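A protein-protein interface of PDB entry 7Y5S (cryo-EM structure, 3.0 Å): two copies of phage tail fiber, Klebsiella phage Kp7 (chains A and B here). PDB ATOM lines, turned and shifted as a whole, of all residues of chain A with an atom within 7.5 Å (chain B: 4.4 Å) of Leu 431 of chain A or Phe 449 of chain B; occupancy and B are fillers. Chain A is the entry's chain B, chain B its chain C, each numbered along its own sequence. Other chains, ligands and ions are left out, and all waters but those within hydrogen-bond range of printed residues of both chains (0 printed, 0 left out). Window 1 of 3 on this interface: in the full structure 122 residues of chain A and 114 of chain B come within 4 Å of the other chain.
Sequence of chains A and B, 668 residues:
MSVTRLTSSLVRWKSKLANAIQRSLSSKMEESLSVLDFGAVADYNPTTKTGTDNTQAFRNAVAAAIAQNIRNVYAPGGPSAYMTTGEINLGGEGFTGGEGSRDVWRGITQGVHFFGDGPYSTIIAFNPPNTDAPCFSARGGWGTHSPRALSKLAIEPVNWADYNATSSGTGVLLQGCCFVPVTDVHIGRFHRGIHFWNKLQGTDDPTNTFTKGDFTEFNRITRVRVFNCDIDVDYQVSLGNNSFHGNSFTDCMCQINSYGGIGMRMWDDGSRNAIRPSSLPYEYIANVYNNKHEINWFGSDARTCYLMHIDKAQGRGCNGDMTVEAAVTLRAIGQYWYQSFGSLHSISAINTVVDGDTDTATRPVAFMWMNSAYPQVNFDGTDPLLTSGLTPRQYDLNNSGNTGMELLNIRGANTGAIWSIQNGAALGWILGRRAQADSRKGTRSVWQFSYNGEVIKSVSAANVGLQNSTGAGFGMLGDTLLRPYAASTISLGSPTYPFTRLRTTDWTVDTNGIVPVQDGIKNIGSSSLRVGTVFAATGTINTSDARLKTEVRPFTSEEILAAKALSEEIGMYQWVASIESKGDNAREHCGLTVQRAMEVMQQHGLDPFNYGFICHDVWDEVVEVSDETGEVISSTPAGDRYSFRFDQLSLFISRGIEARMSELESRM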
ATOM      1  N   TRP A 419     -21.798   0.997  19.242  1.00  0.00           N
ATOM      2  CA  TRP A 419     -22.683   1.085  20.396  1.00  0.00           C
ATOM      3  C   TRP A 419     -21.832   1.349  21.627  1.00  0.00           C
ATOM      4  O   TRP A 419     -20.918   0.577  21.937  1.00  0.00           O
ATOM      5  CB  TRP A 419     -23.552  -0.170  20.545  1.00  0.00           C
ATOM      6  CG  TRP A 419     -22.863  -1.443  20.904  1.00  0.00           C
ATOM      7  CD1 TRP A 419     -22.022  -2.169  20.116  1.00  0.00           C
ATOM      8  CD2 TRP A 419     -23.005  -2.177  22.126  1.00  0.00           C
ATOM      9  NE1 TRP A 419     -21.612  -3.300  20.779  1.00  0.00           N
ATOM     10  CE2 TRP A 419     -22.200  -3.327  22.017  1.00  0.00           C
ATOM     11  CE3 TRP A 419     -23.724  -1.967  23.306  1.00  0.00           C
ATOM     12  CZ2 TRP A 419     -22.092  -4.263  23.043  1.00  0.00           C
ATOM     13  CZ3 TRP A 419     -23.615  -2.897  24.323  1.00  0.00           C
ATOM     14  CH2 TRP A 419     -22.807  -4.031  24.184  1.00  0.00           C
ATOM     15  N   GLY A 428     -18.232  -2.406  31.498  1.00  0.00           N
ATOM     16  CA  GLY A 428     -18.009  -2.476  30.067  1.00  0.00           C
ATOM     17  C   GLY A 428     -19.164  -3.135  29.330  1.00  0.00           C
ATOM     18  O   GLY A 428     -20.322  -3.087  29.753  1.00  0.00           O
ATOM     19  N   TRP A 429     -18.835  -3.763  28.204  1.00  0.00           N
ATOM     20  CA  TRP A 429     -19.816  -4.420  27.351  1.00  0.00           C
ATOM     21  C   TRP A 429     -19.826  -5.910  27.660  1.00  0.00           C
ATOM     22  O   TRP A 429     -18.768  -6.549  27.691  1.00  0.00           O
ATOM     23  CB  TRP A 429     -19.497  -4.189  25.875  1.00  0.00           C
ATOM     24  CG  TRP A 429     -19.311  -2.748  25.529  1.00  0.00           C
ATOM     25  CD1 TRP A 429     -20.241  -1.900  25.003  1.00  0.00           C
ATOM     26  CD2 TRP A 429     -18.109  -1.982  25.677  1.00  0.00           C
ATOM     27  NE1 TRP A 429     -19.694  -0.653  24.819  1.00  0.00           N
ATOM     28  CE2 TRP A 429     -18.386  -0.678  25.226  1.00  0.00           C
ATOM     29  CE3 TRP A 429     -16.826  -2.275  26.149  1.00  0.00           C
ATOM     30  CZ2 TRP A 429     -17.427   0.331  25.234  1.00  0.00           C
ATOM     31  CZ3 TRP A 429     -15.877  -1.270  26.155  1.00  0.00           C
ATOM     32  CH2 TRP A 429     -16.181   0.015  25.701  1.00  0.00           C
ATOM     33  N   ILE A 430     -21.016  -6.459  27.887  1.00  0.00           N
ATOM     34  CA  ILE A 430     -21.173  -7.838  28.327  1.00  0.00           C
ATOM     35  C   ILE A 430     -22.107  -8.570  27.373  1.00  0.00           C
ATOM     36  O   ILE A 430     -23.144  -8.033  26.965  1.00  0.00           O
ATOM     37  CB  ILE A 430     -21.704  -7.917  29.773  1.00  0.00           C
ATOM     38  CG1 ILE A 430     -20.853  -7.051  30.705  1.00  0.00           C
ATOM     39  CG2 ILE A 430     -21.707  -9.357  30.262  1.00  0.00           C
ATOM     40  CD1 ILE A 430     -21.187  -7.217  32.171  1.00  0.00           C
ATOM     41  N   LEU A 431     -21.722  -9.789  27.009  1.00  0.00           N
ATOM     42  CA  LEU A 431     -22.579 -10.732  26.297  1.00  0.00           C
ATOM     43  C   LEU A 431     -23.118 -11.708  27.333  1.00  0.00           C
ATOM     44  O   LEU A 431     -22.342 -12.439  27.959  1.00  0.00           O
ATOM     45  CB  LEU A 431     -21.805 -11.469  25.206  1.00  0.00           C
ATOM     46  CG  LEU A 431     -21.317 -10.681  23.992  1.00  0.00           C
ATOM     47  CD1 LEU A 431     -20.448 -11.557  23.104  1.00  0.00           C
ATOM     48  CD2 LEU A 431     -22.499 -10.162  23.214  1.00  0.00           C
ATOM     49  N   GLY A 432     -24.443 -11.726  27.512  1.00  0.00           N
ATOM     50  CA  GLY A 432     -25.075 -12.527  28.535  1.00  0.00           C
ATOM     51  C   GLY A 432     -26.216 -13.371  27.988  1.00  0.00           C
ATOM     52  O   GLY A 432     -26.635 -13.233  26.835  1.00  0.00           O
ATOM     53  N   ARG A 433     -26.718 -14.257  28.847  1.00  0.00           N
ATOM     54  CA  ARG A 433     -27.813 -15.148  28.493  1.00  0.00           C
ATOM     55  C   ARG A 433     -28.790 -15.226  29.657  1.00  0.00           C
ATOM     56  O   ARG A 433     -28.434 -14.977  30.811  1.00  0.00           O
ATOM     57  CB  ARG A 433     -27.303 -16.546  28.118  1.00  0.00           C
ATOM     58  CG  ARG A 433     -26.442 -17.207  29.183  1.00  0.00           C
ATOM     59  CD  ARG A 433     -26.241 -18.682  28.880  1.00  0.00           C
ATOM     60  NE  ARG A 433     -25.390 -19.340  29.865  1.00  0.00           N
ATOM     61  CZ  ARG A 433     -25.819 -19.829  31.020  1.00  0.00           C
ATOM     62  NH1 ARG A 433     -27.091 -19.749  31.375  1.00  0.00           N
ATOM     63  NH2 ARG A 433     -24.950 -20.414  31.840  1.00  0.00           N
ATOM     64  N   THR A 443     -29.818 -12.953  34.722  1.00  0.00           N
ATOM     65  CA  THR A 443     -29.053 -12.950  33.484  1.00  0.00           C
ATOM     66  C   THR A 443     -27.627 -13.416  33.752  1.00  0.00           C
ATOM     67  O   THR A 443     -26.961 -12.917  34.666  1.00  0.00           O
ATOM     68  CB  THR A 443     -29.049 -11.554  32.863  1.00  0.00           C
ATOM     69  OG1 THR A 443     -30.395 -11.153  32.577  1.00  0.00           O
ATOM     70  CG2 THR A 443     -28.240 -11.543  31.574  1.00  0.00           C
ATOM     71  N   ARG A 444     -27.157 -14.370  32.954  1.00  0.00           N
ATOM     72  CA  ARG A 444     -25.852 -14.984  33.151  1.00  0.00           C
ATOM     73  C   ARG A 444     -24.857 -14.400  32.158  1.00  0.00           C
ATOM     74  O   ARG A 444     -25.026 -14.549  30.943  1.00  0.00           O
ATOM     75  CB  ARG A 444     -25.939 -16.500  32.986  1.00  0.00           C
ATOM     76  CG  ARG A 444     -26.817 -17.180  34.020  1.00  0.00           C
ATOM     77  CD  ARG A 444     -26.195 -17.127  35.403  1.00  0.00           C
ATOM     78  NE  ARG A 444     -26.985 -17.875  36.373  1.00  0.00           N
ATOM     79  CZ  ARG A 444     -27.956 -17.350  37.110  1.00  0.00           C
ATOM     80  NH1 ARG A 444     -28.271 -16.068  37.024  1.00  0.00           N
ATOM     81  NH2 ARG A 444     -28.624 -18.131  37.953  1.00  0.00           N
ATOM     82  N   SER A 445     -23.818 -13.751  32.677  1.00  0.00           N
ATOM     83  CA  SER A 445     -22.796 -13.149  31.831  1.00  0.00           C
ATOM     84  C   SER A 445     -21.903 -14.231  31.239  1.00  0.00           C
ATOM     85  O   SER A 445     -21.485 -15.157  31.940  1.00  0.00           O
ATOM     86  CB  SER A 445     -21.965 -12.151  32.633  1.00  0.00           C
ATOM     87  OG  SER A 445     -21.160 -12.814  33.591  1.00  0.00           O
ATOM     88  N   VAL A 446     -21.610 -14.111  29.948  1.00  0.00           N
ATOM     89  CA  VAL A 446     -20.805 -15.082  29.219  1.00  0.00           C
ATOM     90  C   VAL A 446     -19.494 -14.468  28.737  1.00  0.00           C
ATOM     91  O   VAL A 446     -18.424 -15.053  28.911  1.00  0.00           O
ATOM     92  CB  VAL A 446     -21.601 -15.682  28.039  1.00  0.00           C
ATOM     93  CG1 VAL A 446     -20.780 -16.742  27.328  1.00  0.00           C
ATOM     94  CG2 VAL A 446     -22.921 -16.259  28.527  1.00  0.00           C
ATOM     95  N   TRP A 447     -19.562 -13.287  28.130  1.00  0.00           N
ATOM     96  CA  TRP A 447     -18.395 -12.605  27.587  1.00  0.00           C
ATOM     97  C   TRP A 447     -18.294 -11.207  28.175  1.00  0.00           C
ATOM     98  O   TRP A 447     -19.311 -10.537  28.372  1.00  0.00           O
ATOM     99  CB  TRP A 447     -18.463 -12.504  26.057  1.00  0.00           C
ATOM    100  CG  TRP A 447     -18.264 -13.796  25.333  1.00  0.00           C
ATOM    101  CD1 TRP A 447     -19.233 -14.635  24.867  1.00  0.00           C
ATOM    102  CD2 TRP A 447     -17.012 -14.385  24.964  1.00  0.00           C
ATOM    103  NE1 TRP A 447     -18.663 -15.717  24.242  1.00  0.00           N
ATOM    104  CE2 TRP A 447     -17.299 -15.588  24.289  1.00  0.00           C
ATOM    105  CE3 TRP A 447     -15.675 -14.017  25.146  1.00  0.00           C
ATOM    106  CZ2 TRP A 447     -16.300 -16.421  23.793  1.00  0.00           C
ATOM    107  CZ3 TRP A 447     -14.686 -14.846  24.654  1.00  0.00           C
ATOM    108  CH2 TRP A 447     -15.004 -16.036  23.986  1.00  0.00           C
ATOM    109  N   GLN A 448     -17.067 -10.764  28.437  1.00  0.00           N
ATOM    110  CA  GLN A 448     -16.808  -9.397  28.866  1.00  0.00           C
ATOM    111  C   GLN A 448     -15.687  -8.811  28.025  1.00  0.00           C
ATOM    112  O   GLN A 448     -14.705  -9.495  27.719  1.00  0.00           O
ATOM    113  CB  GLN A 448     -16.440  -9.329  30.352  1.00  0.00           C
ATOM    114  CG  GLN A 448     -16.671  -7.963  30.976  1.00  0.00           C
ATOM    115  CD  GLN A 448     -15.905  -7.768  32.270  1.00  0.00           C
ATOM    116  OE1 GLN A 448     -14.912  -8.450  32.525  1.00  0.00           O
ATOM    117  NE2 GLN A 448     -16.363  -6.835  33.094  1.00  0.00           N
ATOM    118  N   PHE A 449     -15.836  -7.541  27.650  1.00  0.00           N
ATOM    119  CA  PHE A 449     -14.860  -6.857  26.814  1.00  0.00           C
ATOM    120  C   PHE A 449     -14.114  -5.753  27.552  1.00  0.00           C
ATOM    121  O   PHE A 449     -13.209  -5.145  26.967  1.00  0.00           O
ATOM    122  CB  PHE A 449     -15.546  -6.280  25.570  1.00  0.00           C
ATOM    123  CG  PHE A 449     -15.972  -7.322  24.576  1.00  0.00           C
ATOM    124  CD1 PHE A 449     -15.047  -7.922  23.737  1.00  0.00           C
ATOM    125  CD2 PHE A 449     -17.299  -7.706  24.483  1.00  0.00           C
ATOM    126  CE1 PHE A 449     -15.438  -8.882  22.825  1.00  0.00           C
ATOM    127  CE2 PHE A 449     -17.698  -8.665  23.571  1.00  0.00           C
ATOM    128  CZ  PHE A 449     -16.766  -9.254  22.742  1.00  0.00           C
ATOM    129  N   ILE A 456     -10.363  -9.753  27.027  1.00  0.00           N
ATOM    130  CA  ILE A 456     -11.625 -10.371  26.640  1.00  0.00           C
ATOM    131  C   ILE A 456     -11.798 -11.602  27.515  1.00  0.00           C
ATOM    132  O   ILE A 456     -11.036 -12.571  27.396  1.00  0.00           O
ATOM    133  CB  ILE A 456     -11.651 -10.740  25.149  1.00  0.00           C
ATOM    134  CG1 ILE A 456     -11.451  -9.490  24.289  1.00  0.00           C
ATOM    135  CG2 ILE A 456     -12.959 -11.428  24.795  1.00  0.00           C
ATOM    136  CD1 ILE A 456     -11.393  -9.774  22.804  1.00  0.00           C
ATOM    137  N   LYS A 457     -12.793 -11.568  28.395  1.00  0.00           N
ATOM    138  CA  LYS A 457     -12.913 -12.537  29.473  1.00  0.00           C
ATOM    139  C   LYS A 457     -14.167 -13.382  29.296  1.00  0.00           C
ATOM    140  O   LYS A 457     -15.266 -12.853  29.107  1.00  0.00           O
ATOM    141  CB  LYS A 457     -12.949 -11.830  30.833  1.00  0.00           C
ATOM    142  CG  LYS A 457     -13.015 -12.763  32.028  1.00  0.00           C
ATOM    143  CD  LYS A 457     -12.933 -11.981  33.328  1.00  0.00           C
ATOM    144  CE  LYS A 457     -13.147 -12.881  34.532  1.00  0.00           C
ATOM    145  NZ  LYS A 457     -12.043 -13.868  34.676  1.00  0.00           N
ATOM    146  N   VAL A 459     -16.533 -15.005  31.276  1.00  0.00           N
ATOM    147  CA  VAL A 459     -16.829 -14.822  32.695  1.00  0.00           C
ATOM    148  C   VAL A 459     -17.282 -16.130  33.331  1.00  0.00           C
ATOM    149  O   VAL A 459     -16.880 -16.463  34.451  1.00  0.00           O
ATOM    150  CB  VAL A 459     -17.875 -13.709  32.882  1.00  0.00           C
ATOM    151  CG1 VAL A 459     -18.121 -13.461  34.361  1.00  0.00           C
ATOM    152  CG2 VAL A 459     -17.423 -12.435  32.186  1.00  0.00           C
ATOM    153  N   TRP B 419     -26.330  -6.928  26.033  1.00  0.00           N
ATOM    154  CA  TRP B 419     -27.351  -7.392  25.105  1.00  0.00           C
ATOM    155  C   TRP B 419     -27.328  -8.911  25.094  1.00  0.00           C
ATOM    156  O   TRP B 419     -26.291  -9.521  24.815  1.00  0.00           O
ATOM    157  CB  TRP B 419     -27.164  -6.794  23.705  1.00  0.00           C
ATOM    158  CG  TRP B 419     -25.966  -7.225  22.930  1.00  0.00           C
ATOM    159  CD1 TRP B 419     -24.665  -6.913  23.192  1.00  0.00           C
ATOM    160  CD2 TRP B 419     -25.959  -7.999  21.726  1.00  0.00           C
ATOM    161  NE1 TRP B 419     -23.846  -7.463  22.238  1.00  0.00           N
ATOM    162  CE2 TRP B 419     -24.616  -8.137  21.327  1.00  0.00           C
ATOM    163  CE3 TRP B 419     -26.957  -8.600  20.953  1.00  0.00           C
ATOM    164  CZ2 TRP B 419     -24.244  -8.853  20.191  1.00  0.00           C
ATOM    165  CZ3 TRP B 419     -26.586  -9.309  19.824  1.00  0.00           C
ATOM    166  CH2 TRP B 419     -25.241  -9.429  19.454  1.00  0.00           C
ATOM    167  N   TRP B 429     -23.954 -14.937  19.554  1.00  0.00           N
ATOM    168  CA  TRP B 429     -23.926 -13.577  19.032  1.00  0.00           C
ATOM    169  C   TRP B 429     -23.046 -13.541  17.790  1.00  0.00           C
ATOM    170  O   TRP B 429     -21.911 -14.030  17.815  1.00  0.00           O
ATOM    171  CB  TRP B 429     -23.401 -12.600  20.082  1.00  0.00           C
ATOM    172  CG  TRP B 429     -24.117 -12.695  21.390  1.00  0.00           C
ATOM    173  CD1 TRP B 429     -25.148 -11.914  21.822  1.00  0.00           C
ATOM    174  CD2 TRP B 429     -23.846 -13.624  22.445  1.00  0.00           C
ATOM    175  NE1 TRP B 429     -25.540 -12.304  23.079  1.00  0.00           N
ATOM    176  CE2 TRP B 429     -24.755 -13.353  23.484  1.00  0.00           C
ATOM    177  CE3 TRP B 429     -22.922 -14.660  22.610  1.00  0.00           C
ATOM    178  CZ2 TRP B 429     -24.768 -14.080  24.671  1.00  0.00           C
ATOM    179  CZ3 TRP B 429     -22.938 -15.381  23.789  1.00  0.00           C
ATOM    180  CH2 TRP B 429     -23.853 -15.088  24.804  1.00  0.00           C
ATOM    181  N   LEU B 431     -21.580 -11.227  14.388  1.00  0.00           N
ATOM    182  CA  LEU B 431     -21.322  -9.998  13.646  1.00  0.00           C
ATOM    183  C   LEU B 431     -21.368 -10.356  12.166  1.00  0.00           C
ATOM    184  O   LEU B 431     -20.551 -11.155  11.696  1.00  0.00           O
ATOM    185  CB  LEU B 431     -19.966  -9.402  14.019  1.00  0.00           C
ATOM    186  CG  LEU B 431     -19.775  -8.835  15.424  1.00  0.00           C
ATOM    187  CD1 LEU B 431     -18.325  -8.429  15.639  1.00  0.00           C
ATOM    188  CD2 LEU B 431     -20.684  -7.649  15.623  1.00  0.00           C
ATOM    189  N   GLN B 448     -18.199 -14.776  15.191  1.00  0.00           N
ATOM    190  CA  GLN B 448     -19.057 -15.525  16.097  1.00  0.00           C
ATOM    191  C   GLN B 448     -18.414 -15.574  17.473  1.00  0.00           C
ATOM    192  O   GLN B 448     -17.197 -15.739  17.595  1.00  0.00           O
ATOM    193  CB  GLN B 448     -19.313 -16.949  15.587  1.00  0.00           C
ATOM    194  CG  GLN B 448     -20.567 -17.586  16.162  1.00  0.00           C
ATOM    195  CD  GLN B 448     -20.574 -19.094  16.028  1.00  0.00           C
ATOM    196  OE1 GLN B 448     -19.525 -19.721  15.882  1.00  0.00           O
ATOM    197  NE2 GLN B 448     -21.761 -19.689  16.081  1.00  0.00           N
ATOM    198  N   PHE B 449     -19.239 -15.428  18.512  1.00  0.00           N
ATOM    199  CA  PHE B 449     -18.762 -15.419  19.885  1.00  0.00           C
ATOM    200  C   PHE B 449     -19.209 -16.638  20.680  1.00  0.00           C
ATOM    201  O   PHE B 449     -18.810 -16.779  21.841  1.00  0.00           O
ATOM    202  CB  PHE B 449     -19.225 -14.139  20.594  1.00  0.00           C
ATOM    203  CG  PHE B 449     -18.517 -12.899  20.124  1.00  0.00           C
ATOM    204  CD1 PHE B 449     -17.229 -12.617  20.545  1.00  0.00           C
ATOM    205  CD2 PHE B 449     -19.144 -12.018  19.260  1.00  0.00           C
ATOM    206  CE1 PHE B 449     -16.578 -11.477  20.110  1.00  0.00           C
ATOM    207  CE2 PHE B 449     -18.500 -10.876  18.823  1.00  0.00           C
ATOM    208  CZ  PHE B 449     -17.214 -10.606  19.248  1.00  0.00           C
ATOM    209  N   SER B 450     -20.040 -17.503  20.090  1.00  0.00           N
ATOM    210  CA  SER B 450     -20.442 -18.788  20.658  1.00  0.00           C
ATOM    211  C   SER B 450     -21.354 -18.642  21.872  1.00  0.00           C
ATOM    212  O   SER B 450     -21.213 -17.707  22.665  1.00  0.00           O
ATOM    213  CB  SER B 450     -19.213 -19.626  21.026  1.00  0.00           C
ATOM    214  OG  SER B 450     -18.466 -19.960  19.869  1.00  0.00           O
ATOM    215  N   GLY B 453     -19.329 -19.520  25.293  1.00  0.00           N
ATOM    216  CA  GLY B 453     -18.209 -18.673  25.679  1.00  0.00           C
ATOM    217  C   GLY B 453     -16.863 -19.356  25.597  1.00  0.00           C
ATOM    218  O   GLY B 453     -16.060 -19.254  26.530  1.00  0.00           O
ATOM    219  N   VAL B 455     -15.006 -19.998  22.079  1.00  0.00           N
ATOM    220  CA  VAL B 455     -14.194 -19.653  20.918  1.00  0.00           C
ATOM    221  C   VAL B 455     -14.746 -18.387  20.276  1.00  0.00           C
ATOM    222  O   VAL B 455     -15.963 -18.184  20.215  1.00  0.00           O
ATOM    223  CB  VAL B 455     -14.140 -20.805  19.887  1.00  0.00           C
ATOM    224  CG1 VAL B 455     -13.487 -22.037  20.489  1.00  0.00           C
ATOM    225  CG2 VAL B 455     -15.531 -21.145  19.378  1.00  0.00           C
ATOM    226  N   ILE B 456     -13.842 -17.527  19.818  1.00  0.00           N
ATOM    227  CA  ILE B 456     -14.177 -16.399  18.959  1.00  0.00           C
ATOM    228  C   ILE B 456     -13.756 -16.781  17.548  1.00  0.00           C
ATOM    229  O   ILE B 456     -12.558 -16.921  17.266  1.00  0.00           O
ATOM    230  CB  ILE B 456     -13.486 -15.104  19.416  1.00  0.00           C
ATOM    231  CG1 ILE B 456     -13.906 -14.754  20.842  1.00  0.00           C
ATOM    232  CG2 ILE B 456     -13.817 -13.964  18.465  1.00  0.00           C
ATOM    233  CD1 ILE B 456     -13.217 -13.527  21.400  1.00  0.00           C
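The backbone carbonyl oxygen of Ile 430 of chain A lies within hydrogen-bond range of the backbone NH of Trp 419 of chain B (3.5 Å).
NE1 of Trp 447 of chain A is in hydrogen-bond range of O of Phe 449 of chain B (2.6 Å).
The backbone NH (N) of Val 459 of chain A is in hydrogen-bond range of the backbone carbonyl oxygen (O) of Val 446 of chain A (3.0 Å).
The indole nitrogen (NE1) of Trp 429 of chain A is in hydrogen-bond range of the backbone carbonyl oxygen (O) of Trp 419 of chain A, at 3.4 Å.
The backbone carbonyl oxygen (O) of Trp 419 of chain B is in hydrogen-bond range of the indole nitrogen (NE1) of Trp 429 of chain B, 3.4 Å away.
The backbone carbonyl oxygen (O) of Trp 429 of chain A lies within hydrogen-bond range of the backbone NH (N) of Phe 449 of chain A.
The backbone carbonyl oxygen (O) of Leu 431 of chain A is in hydrogen-bond range of the backbone NH (N) of Val 446 of chain A, at 2.7 Å.
OG of Ser 450 of chain B sits at hydrogen-bond distance from O of Val 455 of chain B (3.1 Å).
Among the printed residues, merely in contact across the chains: Trp 419 of chain A with Trp 419 of chain B, Leu 431 of chain A with Trp 419 of chain B, Leu 431 of chain A with Trp 429 of chain B, Leu 431 of chain A with Phe 449 of chain B, Gly 432 of chain A with Trp 419 of chain B, Gly 432 of chain A with Trp 429 of chain B, Val 446 of chain A with Trp 429 of chain B, Val 446 of chain A with Gly 453 of chain B, Trp 447 of chain A with Trp 429 of chain B, Trp 447 of chain A with Ser 450 of chain B, Trp 447 of chain A with Gly 453 of chain B, Trp 447 of chain A with Ile 456 of chain B, Phe 449 of chain A with Phe 449 of chain B and Ile 456 of chain A with Ile 456 of chain B.
Printed residues of chain B within 4 Å of Ile 430 of chain A: Trp 419 (3.5 Å).
Of the printed residues of chain B, Leu 431 of chain A touches Trp 419, Trp 429 and Phe 449.
Printed residues of chain B within 4 Å of Val 446 of chain A: Trp 429 (3.99 Å) and Gly 453 (3.6 Å).
Printed residues of chain B within 4 Å of Phe 449 of chain A: Phe 449.
Of the printed residues of chain A, Trp 419 of chain B touches Trp 419, Ile 430, Leu 431 and Gly 432.
Gln 448 of chain B touches none of the printed residues of chain A.
Phe 449 of chain B touches just these residues of chain A: Leu 431 (3.8 Å), Trp 447 (2.6 Å) and Phe 449 (3.5 Å).
Of the printed residues of chain A, Ser 450 of chain B touches Trp 447.
Among the printed residues, 16 pairs touch across the chains.
Among the printed residues, no Asp or Glu carboxylate lies within 4 Å of a Lys or Arg side-chain nitrogen of the other chain.
Trp 419 of chain B touches its own counterpart, Trp 419 of chain A.
Leu 431 of chain A touches Trp 429 of chain B, but with the chains exchanged Trp 429 of chain A does not touch Leu 431 of chain B (10.9 Å).
Leu 431 of chain A touches Phe 449 of chain B, but with the chains exchanged Phe 449 of chain A does not touch Leu 431 of chain B (7.3 Å).
Phe 449 of chain A touches its own counterpart, Phe 449 of chain B.
Of the 16 pairs that touch across the chains among the printed residues, 3 have their exchanged pair printed and touching as well.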
